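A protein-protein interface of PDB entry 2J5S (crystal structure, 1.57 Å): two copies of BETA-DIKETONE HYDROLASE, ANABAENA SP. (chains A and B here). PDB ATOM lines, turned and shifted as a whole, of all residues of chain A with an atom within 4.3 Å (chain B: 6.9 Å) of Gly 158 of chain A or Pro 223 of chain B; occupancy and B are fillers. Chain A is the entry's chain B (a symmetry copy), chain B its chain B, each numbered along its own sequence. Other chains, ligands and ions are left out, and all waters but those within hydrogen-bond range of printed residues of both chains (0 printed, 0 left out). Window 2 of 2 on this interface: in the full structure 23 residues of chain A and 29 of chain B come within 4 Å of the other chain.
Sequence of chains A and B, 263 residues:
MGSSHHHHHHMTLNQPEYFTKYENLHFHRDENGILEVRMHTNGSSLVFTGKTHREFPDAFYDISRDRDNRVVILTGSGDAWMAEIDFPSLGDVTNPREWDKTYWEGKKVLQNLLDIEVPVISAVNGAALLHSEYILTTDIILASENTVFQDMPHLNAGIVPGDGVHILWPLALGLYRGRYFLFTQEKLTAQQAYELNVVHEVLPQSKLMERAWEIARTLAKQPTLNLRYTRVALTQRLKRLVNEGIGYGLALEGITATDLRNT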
ATOM      1  N   HIS A 154     -22.107 -21.152 -15.814  1.00  0.00           N
ATOM      2  CA  HIS A 154     -21.519 -22.323 -15.207  1.00  0.00           C
ATOM      3  C   HIS A 154     -20.884 -22.033 -13.868  1.00  0.00           C
ATOM      4  O   HIS A 154     -21.264 -22.647 -12.876  1.00  0.00           O
ATOM      5  CB  HIS A 154     -20.523 -22.962 -16.187  1.00  0.00           C
ATOM      6  CG  HIS A 154     -21.190 -23.462 -17.422  1.00  0.00           C
ATOM      7  ND1 HIS A 154     -21.039 -22.849 -18.651  1.00  0.00           N
ATOM      8  CD2 HIS A 154     -22.041 -24.499 -17.613  1.00  0.00           C
ATOM      9  CE1 HIS A 154     -21.736 -23.518 -19.552  1.00  0.00           C
ATOM     10  NE2 HIS A 154     -22.368 -24.509 -18.948  1.00  0.00           N
ATOM     11  N   LEU A 155     -19.940 -21.102 -13.841  1.00  0.00           N
ATOM     12  CA  LEU A 155     -19.308 -20.750 -12.577  1.00  0.00           C
ATOM     13  C   LEU A 155     -20.212 -19.916 -11.653  1.00  0.00           C
ATOM     14  O   LEU A 155     -19.908 -19.821 -10.454  1.00  0.00           O
ATOM     15  CB  LEU A 155     -17.907 -20.144 -12.791  1.00  0.00           C
ATOM     16  CG  LEU A 155     -16.742 -21.165 -12.769  1.00  0.00           C
ATOM     17  CD1 LEU A 155     -16.861 -22.259 -13.812  1.00  0.00           C
ATOM     18  CD2 LEU A 155     -15.442 -20.418 -12.899  1.00  0.00           C
ATOM     19  N   ASN A 156     -21.295 -19.334 -12.190  1.00  0.00           N
ATOM     20  CA  ASN A 156     -22.353 -18.777 -11.332  1.00  0.00           C
ATOM     21  C   ASN A 156     -23.089 -19.857 -10.537  1.00  0.00           C
ATOM     22  O   ASN A 156     -23.467 -19.626  -9.367  1.00  0.00           O
ATOM     23  CB  ASN A 156     -23.355 -17.969 -12.162  1.00  0.00           C
ATOM     24  CG  ASN A 156     -22.855 -16.581 -12.492  1.00  0.00           C
ATOM     25  OD1 ASN A 156     -21.652 -16.253 -12.320  1.00  0.00           O
ATOM     26  ND2 ASN A 156     -23.777 -15.744 -13.006  1.00  0.00           N
ATOM     27  N   ALA A 157     -23.312 -21.009 -11.169  1.00  0.00           N
ATOM     28  CA  ALA A 157     -24.066 -22.111 -10.543  1.00  0.00           C
ATOM     29  C   ALA A 157     -23.146 -23.058  -9.776  1.00  0.00           C
ATOM     30  O   ALA A 157     -23.592 -23.842  -8.925  1.00  0.00           O
ATOM     31  CB  ALA A 157     -24.863 -22.891 -11.611  1.00  0.00           C
ATOM     32  N   GLY A 158     -21.864 -22.995 -10.085  1.00  0.00           N
ATOM     33  CA  GLY A 158     -20.885 -23.871  -9.469  1.00  0.00           C
ATOM     34  C   GLY A 158     -20.723 -25.225 -10.169  1.00  0.00           C
ATOM     35  O   GLY A 158     -20.375 -26.236  -9.513  1.00  0.00           O
ATOM     36  N   ILE A 159     -20.965 -25.244 -11.491  1.00  0.00           N
ATOM     37  CA  ILE A 159     -20.876 -26.497 -12.280  1.00  0.00           C
ATOM     38  C   ILE A 159     -19.879 -26.307 -13.422  1.00  0.00           C
ATOM     39  O   ILE A 159     -19.569 -25.172 -13.794  1.00  0.00           O
ATOM     40  CB  ILE A 159     -22.246 -26.942 -12.814  1.00  0.00           C
ATOM     41  CG1 ILE A 159     -22.807 -25.949 -13.841  1.00  0.00           C
ATOM     42  CG2 ILE A 159     -23.229 -27.177 -11.615  1.00  0.00           C
ATOM     43  CD1 ILE A 159     -24.187 -26.330 -14.444  1.00  0.00           C
ATOM     44  N   THR A 256     -20.809 -32.374 -10.970  1.00  0.00           N
ATOM     45  CA  THR A 256     -20.846 -31.114 -10.216  1.00  0.00           C
ATOM     46  C   THR A 256     -22.278 -30.670  -9.936  1.00  0.00           C
ATOM     47  O   THR A 256     -22.534 -30.064  -8.877  1.00  0.00           O
ATOM     48  CB  THR A 256     -19.993 -29.979 -10.870  1.00  0.00           C
ATOM     49  OG1 THR A 256     -20.430 -29.724 -12.209  1.00  0.00           O
ATOM     50  CG2 THR A 256     -18.549 -30.371 -10.866  1.00  0.00           C
ATOM     51  N   ARG B  70      -6.632 -26.722  -3.294  1.00  0.00           N
ATOM     52  CA  ARG B  70      -7.844 -26.344  -4.054  1.00  0.00           C
ATOM     53  C   ARG B  70      -7.563 -25.367  -5.204  1.00  0.00           C
ATOM     54  O   ARG B  70      -8.294 -25.342  -6.197  1.00  0.00           O
ATOM     55  CB  ARG B  70      -8.942 -25.788  -3.126  1.00  0.00           C
ATOM     56  CG  ARG B  70      -9.315 -26.824  -2.067  1.00  0.00           C
ATOM     57  CD  ARG B  70     -10.423 -26.308  -1.152  1.00  0.00           C
ATOM     58  NE  ARG B  70     -11.692 -26.121  -1.859  1.00  0.00           N
ATOM     59  CZ  ARG B  70     -12.225 -24.957  -2.208  1.00  0.00           C
ATOM     60  NH1 ARG B  70     -11.605 -23.824  -1.947  1.00  0.00           N
ATOM     61  NH2 ARG B  70     -13.397 -24.923  -2.853  1.00  0.00           N
ATOM     62  N   LEU B 219     -11.455 -17.870  -7.152  1.00  0.00           N
ATOM     63  CA  LEU B 219     -11.638 -19.264  -7.573  1.00  0.00           C
ATOM     64  C   LEU B 219     -12.023 -20.156  -6.406  1.00  0.00           C
ATOM     65  O   LEU B 219     -12.893 -21.019  -6.539  1.00  0.00           O
ATOM     66  CB  LEU B 219     -10.344 -19.789  -8.191  1.00  0.00           C
ATOM     67  CG  LEU B 219     -10.188 -19.373  -9.640  1.00  0.00           C
ATOM     68  CD1 LEU B 219      -8.694 -19.566 -10.036  1.00  0.00           C
ATOM     69  CD2 LEU B 219     -11.149 -20.127 -10.601  1.00  0.00           C
ATOM     70  N   ALA B 220     -11.385 -19.935  -5.255  1.00  0.00           N
ATOM     71  CA  ALA B 220     -11.549 -20.830  -4.100  1.00  0.00           C
ATOM     72  C   ALA B 220     -12.968 -20.816  -3.558  1.00  0.00           C
ATOM     73  O   ALA B 220     -13.340 -21.700  -2.788  1.00  0.00           O
ATOM     74  CB  ALA B 220     -10.538 -20.505  -3.005  1.00  0.00           C
ATOM     75  N   LYS B 221     -13.760 -19.829  -3.979  1.00  0.00           N
ATOM     76  CA  LYS B 221     -15.186 -19.762  -3.607  1.00  0.00           C
ATOM     77  C   LYS B 221     -16.025 -20.828  -4.325  1.00  0.00           C
ATOM     78  O   LYS B 221     -17.133 -21.134  -3.903  1.00  0.00           O
ATOM     79  CB  LYS B 221     -15.771 -18.353  -3.871  1.00  0.00           C
ATOM     80  CG  LYS B 221     -15.091 -17.256  -3.034  1.00  0.00           C
ATOM     81  CD  LYS B 221     -15.766 -15.894  -3.264  1.00  0.00           C
ATOM     82  CE  LYS B 221     -15.174 -14.841  -2.338  1.00  0.00           C
ATOM     83  NZ  LYS B 221     -15.594 -13.447  -2.670  1.00  0.00           N
ATOM     84  N   GLN B 222     -15.502 -21.390  -5.420  1.00  0.00           N
ATOM     85  CA  GLN B 222     -16.187 -22.473  -6.137  1.00  0.00           C
ATOM     86  C   GLN B 222     -16.219 -23.721  -5.291  1.00  0.00           C
ATOM     87  O   GLN B 222     -15.304 -23.909  -4.503  1.00  0.00           O
ATOM     88  CB  GLN B 222     -15.434 -22.813  -7.442  1.00  0.00           C
ATOM     89  CG  GLN B 222     -15.526 -21.701  -8.489  1.00  0.00           C
ATOM     90  CD  GLN B 222     -16.954 -21.518  -8.998  1.00  0.00           C
ATOM     91  OE1 GLN B 222     -17.691 -22.491  -9.204  1.00  0.00           O
ATOM     92  NE2 GLN B 222     -17.349 -20.262  -9.212  1.00  0.00           N
ATOM     93  N   PRO B 223     -17.228 -24.608  -5.497  1.00  0.00           N
ATOM     94  CA  PRO B 223     -17.189 -25.935  -4.870  1.00  0.00           C
ATOM     95  C   PRO B 223     -15.938 -26.693  -5.339  1.00  0.00           C
ATOM     96  O   PRO B 223     -15.481 -26.484  -6.463  1.00  0.00           O
ATOM     97  CB  PRO B 223     -18.442 -26.636  -5.413  1.00  0.00           C
ATOM     98  CG  PRO B 223     -19.334 -25.576  -5.930  1.00  0.00           C
ATOM     99  CD  PRO B 223     -18.436 -24.422  -6.324  1.00  0.00           C
ATOM    100  N   THR B 224     -15.389 -27.543  -4.481  1.00  0.00           N
ATOM    101  CA  THR B 224     -14.139 -28.248  -4.781  1.00  0.00           C
ATOM    102  C   THR B 224     -14.238 -29.104  -6.040  1.00  0.00           C
ATOM    103  O   THR B 224     -13.346 -29.033  -6.882  1.00  0.00           O
ATOM    104  CB  THR B 224     -13.713 -29.074  -3.555  1.00  0.00           C
ATOM    105  OG1 THR B 224     -13.532 -28.150  -2.481  1.00  0.00           O
ATOM    106  CG2 THR B 224     -12.427 -29.844  -3.795  1.00  0.00           C
ATOM    107  N   LEU B 225     -15.308 -29.879  -6.178  1.00  0.00           N
ATOM    108  CA  LEU B 225     -15.416 -30.731  -7.385  1.00  0.00           C
ATOM    109  C   LEU B 225     -15.485 -29.871  -8.637  1.00  0.00           C
ATOM    110  O   LEU B 225     -14.955 -30.265  -9.685  1.00  0.00           O
ATOM    111  CB  LEU B 225     -16.620 -31.669  -7.340  1.00  0.00           C
ATOM    112  CG  LEU B 225     -16.444 -32.856  -6.375  1.00  0.00           C
ATOM    113  CD1 LEU B 225     -17.632 -33.790  -6.497  1.00  0.00           C
ATOM    114  CD2 LEU B 225     -15.120 -33.584  -6.586  1.00  0.00           C
ATOM    115  N   ASN B 226     -16.116 -28.698  -8.550  1.00  0.00           N
ATOM    116  CA  ASN B 226     -16.117 -27.821  -9.713  1.00  0.00           C
ATOM    117  C   ASN B 226     -14.721 -27.342 -10.096  1.00  0.00           C
ATOM    118  O   ASN B 226     -14.365 -27.312 -11.288  1.00  0.00           O
ATOM    119  CB  ASN B 226     -17.074 -26.641  -9.604  1.00  0.00           C
ATOM    120  CG  ASN B 226     -17.380 -26.074 -10.978  1.00  0.00           C
ATOM    121  OD1 ASN B 226     -17.417 -26.828 -11.952  1.00  0.00           O
ATOM    122  ND2 ASN B 226     -17.563 -24.766 -11.072  1.00  0.00           N
ATOM    123  N   LEU B 227     -13.894 -26.972  -9.106  1.00  0.00           N
ATOM    124  CA  LEU B 227     -12.518 -26.574  -9.404  1.00  0.00           C
ATOM    125  C   LEU B 227     -11.789 -27.730 -10.079  1.00  0.00           C
ATOM    126  O   LEU B 227     -11.077 -27.546 -11.084  1.00  0.00           O
ATOM    127  CB  LEU B 227     -11.792 -26.204  -8.111  1.00  0.00           C
ATOM    128  CG  LEU B 227     -12.307 -24.873  -7.544  1.00  0.00           C
ATOM    129  CD1 LEU B 227     -11.727 -24.699  -6.120  1.00  0.00           C
ATOM    130  CD2 LEU B 227     -11.901 -23.704  -8.446  1.00  0.00           C
ATOM    131  N   ARG B 228     -11.963 -28.922  -9.515  1.00  0.00           N
ATOM    132  CA  ARG B 228     -11.231 -30.103 -10.005  1.00  0.00           C
ATOM    133  C   ARG B 228     -11.662 -30.478 -11.407  1.00  0.00           C
ATOM    134  O   ARG B 228     -10.809 -30.685 -12.294  1.00  0.00           O
ATOM    135  CB  ARG B 228     -11.398 -31.269  -9.021  1.00  0.00           C
ATOM    136  CG  ARG B 228     -10.730 -30.925  -7.663  1.00  0.00           C
ATOM    137  CD  ARG B 228     -10.958 -32.053  -6.677  1.00  0.00           C
ATOM    138  NE  ARG B 228     -10.192 -33.256  -7.024  1.00  0.00           N
ATOM    139  CZ  ARG B 228      -8.891 -33.443  -6.758  1.00  0.00           C
ATOM    140  NH1 ARG B 228      -8.171 -32.525  -6.110  1.00  0.00           N
ATOM    141  NH2 ARG B 228      -8.301 -34.572  -7.144  1.00  0.00           N
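Asn 226 of chain B touches Leu 155 of chain A.
Gly 158 of chain A touches Gln 222 of chain B (CA to OE1, 3.5 Å).
Pro 223 of chain B touches Gly 158 of chain A (CG to O, 3.8 Å).
Gly 158 of chain A touches Asn 226 of chain B (C to ND2, 3.3 Å).
Leu 225 of chain B touches Thr 256 of chain A.
Thr 256 of chain A touches Asn 226 of chain B (CG2 to CA, 3.7 Å).
Gly 158 of chain A touches just these residues of chain B: Gln 222 (3.5 Å), Pro 223 (3.8 Å) and Asn 226 (3.3 Å).
Of chain A, only Gly 158 (3.8 Å) comes within 4 Å of Pro 223 of chain B.
Of the printed residues of chain A, Asn 226 of chain B touches Leu 155, Gly 158, Ile 159 and Thr 256.
Printed residues of chain B within 4 Å of Thr 256 of chain A: Leu 225 and Asn 226.
The nearest residue of chain B that does not touch Gly 158 of chain A is Leu 225 of chain B (6.2 Å).
The nearest printed residue of chain A that does not touch Pro 223 of chain B is Ala 157 of chain A (5.5 Å).
The nearest printed residue of chain B that does not touch Ile 159 of chain A is Gln 222 of chain B (4.9 Å).
The guanidinium group (NH2) of Arg 70 of chain B is in hydrogen-bond range of the backbone carbonyl oxygen (O) of Gln 222 of chain B.
OE1 of Gln 222 of chain B is in hydrogen-bond range of ND2 of Asn 226 of chain B.
O of His 154 of chain A is in hydrogen-bond range of N of Ile 159 of chain A.
The side-chain amide nitrogen (NE2) of Gln 222 of chain B sits at hydrogen-bond distance from the backbone carbonyl oxygen (O) of Leu 155 of chain A, at 2.9 Å.
OD1 of Asn 226 of chain B lies close to O of Ile 159 of chain A (3.3 Å).
No position is printed for both chains.
Of the 8 pairs that touch across the chains among the printed residues, none has its exchanged pair printed and touching as well.
Of the 11 printed residues of chain B, 4 touch a printed residue of chain A.
Printed residues of chain B that touch a printed residue of chain A: Gln 222, Pro 223, Leu 225 and Asn 226.
Among the printed residues, 8 pairs touch across the chains.
Among the printed residues, no Asp or Glu carboxylate lies within 4 Å of a Lys or Arg side-chain nitrogen of the other chain.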
